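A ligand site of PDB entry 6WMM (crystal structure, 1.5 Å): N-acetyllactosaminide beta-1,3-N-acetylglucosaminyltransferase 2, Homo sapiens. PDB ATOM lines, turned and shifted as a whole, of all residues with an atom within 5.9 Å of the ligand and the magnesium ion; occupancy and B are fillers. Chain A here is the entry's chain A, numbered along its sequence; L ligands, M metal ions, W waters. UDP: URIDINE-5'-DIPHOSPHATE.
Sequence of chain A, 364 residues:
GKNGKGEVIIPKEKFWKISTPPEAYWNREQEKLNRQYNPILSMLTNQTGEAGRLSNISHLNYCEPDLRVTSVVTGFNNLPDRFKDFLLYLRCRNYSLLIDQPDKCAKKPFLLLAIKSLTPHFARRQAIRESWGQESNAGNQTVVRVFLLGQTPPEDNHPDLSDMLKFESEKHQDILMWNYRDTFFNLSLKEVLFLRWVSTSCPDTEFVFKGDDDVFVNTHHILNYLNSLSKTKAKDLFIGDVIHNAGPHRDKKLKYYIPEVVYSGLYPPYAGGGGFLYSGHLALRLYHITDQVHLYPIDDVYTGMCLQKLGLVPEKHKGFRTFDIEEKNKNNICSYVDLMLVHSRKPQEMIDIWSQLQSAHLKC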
ATOM      1  N   ILE A 115      30.979 -31.366   1.532  1.00  0.00           N
ATOM      2  CA  ILE A 115      30.685 -30.095   0.837  1.00  0.00           C
ATOM      3  C   ILE A 115      29.536 -29.426   1.546  1.00  0.00           C
ATOM      4  O   ILE A 115      28.433 -29.999   1.618  1.00  0.00           O
ATOM      5  CB  ILE A 115      30.337 -30.360  -0.630  1.00  0.00           C
ATOM      6  CG1 ILE A 115      31.514 -31.062  -1.323  1.00  0.00           C
ATOM      7  CG2 ILE A 115      29.962 -29.039  -1.298  1.00  0.00           C
ATOM      8  CD1 ILE A 115      31.323 -32.489  -1.497  1.00  0.00           C
ATOM      9  N   LYS A 116      29.760 -28.187   2.018  1.00  0.00           N
ATOM     10  CA  LYS A 116      28.699 -27.392   2.663  1.00  0.00           C
ATOM     11  C   LYS A 116      27.689 -26.975   1.616  1.00  0.00           C
ATOM     12  O   LYS A 116      28.076 -26.445   0.555  1.00  0.00           O
ATOM     13  CB  LYS A 116      29.299 -26.131   3.317  1.00  0.00           C
ATOM     14  CG  LYS A 116      30.304 -26.487   4.440  1.00  0.00           C
ATOM     15  CD  LYS A 116      31.498 -25.505   4.466  1.00  0.00           C
ATOM     16  CE  LYS A 116      31.022 -24.089   4.719  1.00  0.00           C
ATOM     17  NZ  LYS A 116      32.199 -23.163   4.531  1.00  0.00           N
ATOM     18  N   SER A 117      26.412 -27.165   1.931  1.00  0.00           N
ATOM     19  CA  SER A 117      25.392 -26.761   0.961  1.00  0.00           C
ATOM     20  C   SER A 117      24.132 -26.319   1.693  1.00  0.00           C
ATOM     21  O   SER A 117      23.958 -26.524   2.885  1.00  0.00           O
ATOM     22  CB  SER A 117      25.100 -27.896  -0.021  1.00  0.00           C
ATOM     23  OG  SER A 117      24.368 -27.408  -1.191  1.00  0.00           O
ATOM     24  N   LEU A 118      23.190 -25.725   0.929  1.00  0.00           N
ATOM     25  CA  LEU A 118      21.907 -25.283   1.437  1.00  0.00           C
ATOM     26  C   LEU A 118      20.838 -26.027   0.641  1.00  0.00           C
ATOM     27  O   LEU A 118      21.064 -26.247  -0.571  1.00  0.00           O
ATOM     28  CB  LEU A 118      21.666 -23.763   1.260  1.00  0.00           C
ATOM     29  CG  LEU A 118      22.266 -22.783   2.300  1.00  0.00           C
ATOM     30  CD1 LEU A 118      22.311 -21.316   1.819  1.00  0.00           C
ATOM     31  CD2 LEU A 118      21.478 -22.902   3.585  1.00  0.00           C
ATOM     32  N   HIS A 121      20.133 -25.614  -3.296  1.00  0.00           N
ATOM     33  CA  HIS A 121      21.245 -25.627  -4.250  1.00  0.00           C
ATOM     34  C   HIS A 121      21.343 -26.970  -4.984  1.00  0.00           C
ATOM     35  O   HIS A 121      22.418 -27.625  -5.039  1.00  0.00           O
ATOM     36  CB  HIS A 121      22.562 -25.343  -3.485  1.00  0.00           C
ATOM     37  CG  HIS A 121      22.646 -23.958  -2.899  1.00  0.00           C
ATOM     38  ND1 HIS A 121      23.762 -23.577  -2.163  1.00  0.00           N
ATOM     39  CD2 HIS A 121      21.811 -22.882  -2.910  1.00  0.00           C
ATOM     40  CE1 HIS A 121      23.610 -22.316  -1.779  1.00  0.00           C
ATOM     41  NE2 HIS A 121      22.424 -21.882  -2.190  1.00  0.00           N
ATOM     42  N   ARG A 124      23.976 -26.970  -8.012  1.00  0.00           N
ATOM     43  CA  ARG A 124      25.359 -27.035  -7.505  1.00  0.00           C
ATOM     44  C   ARG A 124      25.729 -28.443  -7.077  1.00  0.00           C
ATOM     45  O   ARG A 124      26.773 -28.950  -7.495  1.00  0.00           O
ATOM     46  CB  ARG A 124      25.560 -26.061  -6.329  1.00  0.00           C
ATOM     47  CG  ARG A 124      25.560 -24.572  -6.700  1.00  0.00           C
ATOM     48  CD  ARG A 124      25.800 -23.769  -5.424  1.00  0.00           C
ATOM     49  NE  ARG A 124      25.886 -22.338  -5.788  1.00  0.00           N
ATOM     50  CZ  ARG A 124      26.201 -21.348  -4.956  1.00  0.00           C
ATOM     51  NH1 ARG A 124      26.499 -21.608  -3.707  1.00  0.00           N
ATOM     52  NH2 ARG A 124      26.253 -20.083  -5.396  1.00  0.00           N
ATOM     53  N   LEU A 148      26.578 -31.399   3.323  1.00  0.00           N
ATOM     54  CA  LEU A 148      26.346 -31.027   4.730  1.00  0.00           C
ATOM     55  C   LEU A 148      25.277 -29.949   4.736  1.00  0.00           C
ATOM     56  O   LEU A 148      25.561 -28.795   4.402  1.00  0.00           O
ATOM     57  CB  LEU A 148      27.617 -30.471   5.378  1.00  0.00           C
ATOM     58  CG  LEU A 148      28.867 -31.359   5.280  1.00  0.00           C
ATOM     59  CD1 LEU A 148      30.096 -30.640   5.914  1.00  0.00           C
ATOM     60  CD2 LEU A 148      28.615 -32.779   5.875  1.00  0.00           C
ATOM     61  N   ASP A 182      19.926 -23.523   9.217  1.00  0.00           N
ATOM     62  CA  ASP A 182      21.135 -23.359   8.403  1.00  0.00           C
ATOM     63  C   ASP A 182      21.274 -21.871   8.046  1.00  0.00           C
ATOM     64  O   ASP A 182      20.493 -21.332   7.265  1.00  0.00           O
ATOM     65  CB  ASP A 182      21.020 -24.238   7.162  1.00  0.00           C
ATOM     66  CG  ASP A 182      22.374 -24.588   6.517  1.00  0.00           C
ATOM     67  OD1 ASP A 182      23.351 -23.818   6.700  1.00  0.00           O
ATOM     68  OD2 ASP A 182      22.395 -25.588   5.772  1.00  0.00           O
ATOM     69  N   THR A 183      22.252 -21.205   8.627  1.00  0.00           N
ATOM     70  CA  THR A 183      22.527 -19.786   8.415  1.00  0.00           C
ATOM     71  C   THR A 183      24.039 -19.578   8.396  1.00  0.00           C
ATOM     72  O   THR A 183      24.804 -20.422   8.873  1.00  0.00           O
ATOM     73  CB  THR A 183      21.970 -18.909   9.541  1.00  0.00           C
ATOM     74  OG1 THR A 183      22.654 -19.234  10.762  1.00  0.00           O
ATOM     75  CG2 THR A 183      20.499 -19.182   9.766  1.00  0.00           C
ATOM     76  N   PHE A 184      24.475 -18.409   7.929  1.00  0.00           N
ATOM     77  CA  PHE A 184      25.922 -18.175   7.926  1.00  0.00           C
ATOM     78  C   PHE A 184      26.500 -18.281   9.320  1.00  0.00           C
ATOM     79  O   PHE A 184      27.587 -18.850   9.498  1.00  0.00           O
ATOM     80  CB  PHE A 184      26.205 -16.798   7.339  1.00  0.00           C
ATOM     81  CG  PHE A 184      26.173 -16.785   5.826  1.00  0.00           C
ATOM     82  CD1 PHE A 184      27.242 -17.301   5.105  1.00  0.00           C
ATOM     83  CD2 PHE A 184      25.068 -16.321   5.150  1.00  0.00           C
ATOM     84  CE1 PHE A 184      27.221 -17.279   3.688  1.00  0.00           C
ATOM     85  CE2 PHE A 184      25.039 -16.327   3.728  1.00  0.00           C
ATOM     86  CZ  PHE A 184      26.132 -16.812   3.029  1.00  0.00           C
ATOM     87  N   LEU A 187      27.371 -21.692  10.710  1.00  0.00           N
ATOM     88  CA  LEU A 187      28.313 -22.568  10.008  1.00  0.00           C
ATOM     89  C   LEU A 187      29.326 -23.197  10.950  1.00  0.00           C
ATOM     90  O   LEU A 187      29.817 -24.286  10.637  1.00  0.00           O
ATOM     91  CB  LEU A 187      29.002 -21.808   8.848  1.00  0.00           C
ATOM     92  CG  LEU A 187      28.083 -21.711   7.622  1.00  0.00           C
ATOM     93  CD1 LEU A 187      28.809 -20.803   6.615  1.00  0.00           C
ATOM     94  CD2 LEU A 187      27.801 -23.119   7.022  1.00  0.00           C
ATOM     95  N   LYS A 190      27.665 -26.190  11.856  1.00  0.00           N
ATOM     96  CA  LYS A 190      27.802 -27.167  10.783  1.00  0.00           C
ATOM     97  C   LYS A 190      29.154 -27.885  10.846  1.00  0.00           C
ATOM     98  O   LYS A 190      29.215 -29.109  10.666  1.00  0.00           O
ATOM     99  CB  LYS A 190      27.576 -26.488   9.409  1.00  0.00           C
ATOM    100  CG  LYS A 190      27.637 -27.471   8.215  1.00  0.00           C
ATOM    101  CD  LYS A 190      27.150 -26.826   6.864  1.00  0.00           C
ATOM    102  CE  LYS A 190      25.653 -26.478   6.946  1.00  0.00           C
ATOM    103  NZ  LYS A 190      25.067 -26.197   5.542  1.00  0.00           N
ATOM    104  N   GLY A 211      34.734 -28.309   1.864  1.00  0.00           N
ATOM    105  CA  GLY A 211      34.699 -27.135   1.012  1.00  0.00           C
ATOM    106  C   GLY A 211      33.292 -26.701   0.705  1.00  0.00           C
ATOM    107  O   GLY A 211      32.328 -27.283   1.192  1.00  0.00           O
ATOM    108  N   ASP A 212      33.200 -25.646  -0.107  1.00  0.00           N
ATOM    109  CA  ASP A 212      31.947 -24.990  -0.422  1.00  0.00           C
ATOM    110  C   ASP A 212      31.364 -25.551  -1.713  1.00  0.00           C
ATOM    111  O   ASP A 212      32.059 -26.162  -2.522  1.00  0.00           O
ATOM    112  CB  ASP A 212      32.181 -23.483  -0.540  1.00  0.00           C
ATOM    113  CG  ASP A 212      32.574 -22.862   0.781  1.00  0.00           C
ATOM    114  OD1 ASP A 212      32.507 -23.560   1.841  1.00  0.00           O
ATOM    115  OD2 ASP A 212      32.902 -21.668   0.759  1.00  0.00           O
ATOM    116  N   ASP A 213      30.074 -25.299  -1.926  1.00  0.00           N
ATOM    117  CA  ASP A 213      29.457 -25.883  -3.108  1.00  0.00           C
ATOM    118  C   ASP A 213      29.511 -24.977  -4.331  1.00  0.00           C
ATOM    119  O   ASP A 213      28.832 -25.244  -5.318  1.00  0.00           O
ATOM    120  CB  ASP A 213      27.986 -26.328  -2.822  1.00  0.00           C
ATOM    121  CG  ASP A 213      27.053 -25.168  -2.483  1.00  0.00           C
ATOM    122  OD1 ASP A 213      27.452 -23.981  -2.416  1.00  0.00           O
ATOM    123  OD2 ASP A 213      25.840 -25.439  -2.223  1.00  0.00           O
ATOM    124  N   ASP A 214      30.305 -23.901  -4.293  1.00  0.00           N
ATOM    125  CA  ASP A 214      30.531 -23.012  -5.423  1.00  0.00           C
ATOM    126  C   ASP A 214      32.006 -22.951  -5.811  1.00  0.00           C
ATOM    127  O   ASP A 214      32.416 -21.970  -6.460  1.00  0.00           O
ATOM    128  CB  ASP A 214      30.019 -21.595  -5.122  1.00  0.00           C
ATOM    129  CG  ASP A 214      30.760 -20.917  -3.952  1.00  0.00           C
ATOM    130  OD1 ASP A 214      31.537 -21.593  -3.276  1.00  0.00           O
ATOM    131  OD2 ASP A 214      30.578 -19.678  -3.725  1.00  0.00           O
ATOM    132  N   LYS A 255      30.037  -8.457   5.123  1.00  0.00           N
ATOM    133  CA  LYS A 255      29.462  -9.773   5.418  1.00  0.00           C
ATOM    134  C   LYS A 255      30.041 -10.356   6.699  1.00  0.00           C
ATOM    135  O   LYS A 255      29.322 -10.960   7.512  1.00  0.00           O
ATOM    136  CB  LYS A 255      29.690 -10.689   4.231  1.00  0.00           C
ATOM    137  CG  LYS A 255      29.173 -12.106   4.367  1.00  0.00           C
ATOM    138  CD  LYS A 255      29.415 -12.819   3.046  1.00  0.00           C
ATOM    139  CE  LYS A 255      28.885 -14.252   3.026  1.00  0.00           C
ATOM    140  NZ  LYS A 255      28.699 -14.744   1.604  1.00  0.00           N
ATOM    141  N   TYR A 256      31.356 -10.220   6.901  1.00  0.00           N
ATOM    142  CA  TYR A 256      31.993 -10.778   8.082  1.00  0.00           C
ATOM    143  C   TYR A 256      32.219  -9.743   9.178  1.00  0.00           C
ATOM    144  O   TYR A 256      33.126  -9.879   9.992  1.00  0.00           O
ATOM    145  CB  TYR A 256      33.271 -11.490   7.652  1.00  0.00           C
ATOM    146  CG  TYR A 256      32.945 -12.667   6.769  1.00  0.00           C
ATOM    147  CD1 TYR A 256      32.245 -13.756   7.274  1.00  0.00           C
ATOM    148  CD2 TYR A 256      33.278 -12.667   5.417  1.00  0.00           C
ATOM    149  CE1 TYR A 256      31.917 -14.864   6.469  1.00  0.00           C
ATOM    150  CE2 TYR A 256      32.941 -13.759   4.600  1.00  0.00           C
ATOM    151  CZ  TYR A 256      32.276 -14.853   5.128  1.00  0.00           C
ATOM    152  OH  TYR A 256      31.948 -15.939   4.319  1.00  0.00           O
ATOM    153  N   GLY A 273      38.167 -19.262   2.616  1.00  0.00           N
ATOM    154  CA  GLY A 273      38.070 -18.943   1.209  1.00  0.00           C
ATOM    155  C   GLY A 273      37.421 -19.991   0.312  1.00  0.00           C
ATOM    156  O   GLY A 273      37.233 -19.711  -0.884  1.00  0.00           O
ATOM    157  N   HIS A 343      37.735 -20.485  -6.498  1.00  0.00           N
ATOM    158  CA  HIS A 343      36.483 -19.885  -6.132  1.00  0.00           C
ATOM    159  C   HIS A 343      36.279 -18.684  -7.030  1.00  0.00           C
ATOM    160  O   HIS A 343      37.187 -17.944  -7.173  1.00  0.00           O
ATOM    161  CB  HIS A 343      36.605 -19.387  -4.704  1.00  0.00           C
ATOM    162  CG  HIS A 343      35.383 -18.710  -4.184  1.00  0.00           C
ATOM    163  ND1 HIS A 343      35.185 -17.372  -4.314  1.00  0.00           N
ATOM    164  CD2 HIS A 343      34.341 -19.186  -3.486  1.00  0.00           C
ATOM    165  CE1 HIS A 343      34.045 -17.047  -3.749  1.00  0.00           C
ATOM    166  NE2 HIS A 343      33.508 -18.133  -3.234  1.00  0.00           N
ATOM    167  N   SER A 344      35.111 -18.486  -7.615  1.00  0.00           N
ATOM    168  CA  SER A 344      33.920 -19.386  -7.532  1.00  0.00           C
ATOM    169  C   SER A 344      33.498 -19.775  -8.961  1.00  0.00           C
ATOM    170  O   SER A 344      33.795 -19.049  -9.917  1.00  0.00           O
ATOM    171  CB  SER A 344      32.746 -18.672  -6.851  1.00  0.00           C
ATOM    172  OG  SER A 344      32.384 -17.483  -7.565  1.00  0.00           O
HETATM  173  N1  UDP L   1      26.361 -21.993   3.097  1.00  0.00           N
HETATM  174  C2  UDP L   1      25.735 -22.835   3.999  1.00  0.00           C
HETATM  175  N3  UDP L   1      24.784 -22.344   4.829  1.00  0.00           N
HETATM  176  C4  UDP L   1      24.498 -21.008   4.838  1.00  0.00           C
HETATM  177  C5  UDP L   1      25.193 -20.130   3.918  1.00  0.00           C
HETATM  178  C6  UDP L   1      26.124 -20.638   3.098  1.00  0.00           C
HETATM  179  O2  UDP L   1      26.037 -24.044   4.022  1.00  0.00           O
HETATM  180  O4  UDP L   1      23.582 -20.571   5.566  1.00  0.00           O
HETATM  181  C1' UDP L   1      27.418 -22.550   2.281  1.00  0.00           C
HETATM  182  C2' UDP L   1      27.283 -22.162   0.798  1.00  0.00           C
HETATM  183  O2' UDP L   1      26.462 -23.145   0.193  1.00  0.00           O
HETATM  184  C3' UDP L   1      28.752 -22.346   0.371  1.00  0.00           C
HETATM  185  C4' UDP L   1      29.501 -21.818   1.592  1.00  0.00           C
HETATM  186  O4' UDP L   1      28.644 -21.919   2.732  1.00  0.00           O
HETATM  187  O3' UDP L   1      29.056 -23.751   0.313  1.00  0.00           O
HETATM  188  C5' UDP L   1      30.006 -20.394   1.385  1.00  0.00           C
HETATM  189  O5' UDP L   1      28.922 -19.537   1.140  1.00  0.00           O
HETATM  190  PA  UDP L   1      29.225 -18.214   0.320  1.00  0.00           P
HETATM  191  O1A UDP L   1      29.686 -18.532  -1.058  1.00  0.00           O
HETATM  192  O2A UDP L   1      27.907 -17.354   0.293  1.00  0.00           O
HETATM  193  O3A UDP L   1      30.379 -17.479   1.089  1.00  0.00           O
HETATM  194  PB  UDP L   1      31.602 -16.617   0.582  1.00  0.00           P
HETATM  195  O1B UDP L   1      32.569 -16.350   1.822  1.00  0.00           O
HETATM  196  O2B UDP L   1      32.408 -17.371  -0.572  1.00  0.00           O
HETATM  197  O3B UDP L   1      30.983 -15.327   0.097  1.00  0.00           O
HETATM  198 MG    MG M   1      31.527 -18.373  -2.028  1.00  0.00          MG
HETATM  199  O   HOH W   1      21.917 -18.473   4.720  1.00  0.00           O
HETATM  200  O   HOH W   2      27.131 -16.302  -1.897  1.00  0.00           O
HETATM  201  O   HOH W   3      27.399 -19.457  -2.384  1.00  0.00           O
HETATM  202  O   HOH W   4      25.360 -19.327  -0.267  1.00  0.00           O
HETATM  203  O   HOH W   5      30.811 -16.801  -3.170  1.00  0.00           O
HETATM  204  O   HOH W   6      32.416 -20.151  -1.319  1.00  0.00           O
HETATM  205  O   HOH W   7      35.213 -15.399   1.947  1.00  0.00           O
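The side-chain hydroxyl (OH) of Tyr 256 sits at hydrogen-bond distance from an oxygen (O1B) of the ligand (2.6 Å).
O3B of the ligand lies within salt-bridge range of NZ of Lys 255, at 2.8 Å.
N of Thr 183 lies close to O4 of the ligand, 3.4 Å away.
The backbone carbonyl oxygen of Lys 116 lies within hydrogen-bond range of an oxygen (O3') of the ligand.
The side-chain amino group of Lys 190 is in hydrogen-bond range of an oxygen (O2) of the ligand.
OD1 of Asp 182 sits at hydrogen-bond distance from N3 of the ligand (2.8 Å).
The backbone NH of Asp 213 sits at hydrogen-bond distance from an oxygen (O3') of the ligand, 2.9 Å away.
The side-chain carboxylate of Asp 213 sits at hydrogen-bond distance from an oxygen (O2') of the ligand, 2.9 Å away.
N of Phe 184 is in hydrogen-bond range of O4 of the ligand, at 3.3 Å.
Water W6 lies within hydrogen-bond range of the side-chain carboxylate (OD1) of Asp 214 (2.6 Å) and the side-chain carboxylate (OD2) of Asp 212 (2.6 Å).
Water W3 lies within hydrogen-bond range of the guanidinium group of Arg 124 (2.7 Å) and an oxygen (O2A) of the ligand (3.4 Å).
O of Lys 116 sits close to N of Asp 213 (3.4 Å).
The side-chain amino group (NZ) of Lys 190 is in hydrogen-bond range of the backbone carbonyl oxygen (O) of Leu 148 (2.9 Å).
The side-chain carboxylate (OD2) of Asp 213 lies within hydrogen-bond range of the side-chain hydroxyl (OG) of Ser 117 (2.7 Å).
OD1 of Asp 212 lies within salt-bridge range of NZ of Lys 116 (2.7 Å).
O of Leu 148 sits at hydrogen-bond distance from N of Ser 117.
The side-chain amino group (NZ) of Lys 190 sits at hydrogen-bond distance from the backbone carbonyl oxygen (O) of Ser 117 (2.9 Å).
O of Gly 211 is in hydrogen-bond range of N of Lys 116, 2.8 Å away.
The side-chain carboxylate (OD1) of Asp 213 lies within salt-bridge range of the guanidinium group (NH1) of Arg 124 (2.9 Å).
The backbone carbonyl oxygen (O) of Ser 117 sits close to an oxygen (O2) of the ligand, at 3.4 Å.
CD2 of Leu 118 touches N3 of the ligand, 3.6 Å away.
His 121 touches the ligand.
Leu 187 touches the ligand (CD2 to O2, 3.6 Å).
Asp 212 touches the ligand.
Hydrophobic or aromatic side chains that line the ligand: Leu 118, His 121, Phe 184, Leu 187, Tyr 256 and His 343.
Of the 21 residues printed, 15 come within 4 Å of the ligand.
Two residues have an atom within 4 Å of the magnesium ion: Asp 214 and His 343.
O2B of the ligand is bound to the magnesium ion (2.0 Å).
The magnesium ion is bound by water W5.
O1A of the ligand binds the magnesium ion (2.1 Å).
Water W6 is bound to the magnesium ion.
NE2 of His 343 is bound to the magnesium ion (2.3 Å).
The magnesium ion is bound by OD2 of Asp 214.
The magnesium ion has six donor atoms within binding distance.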
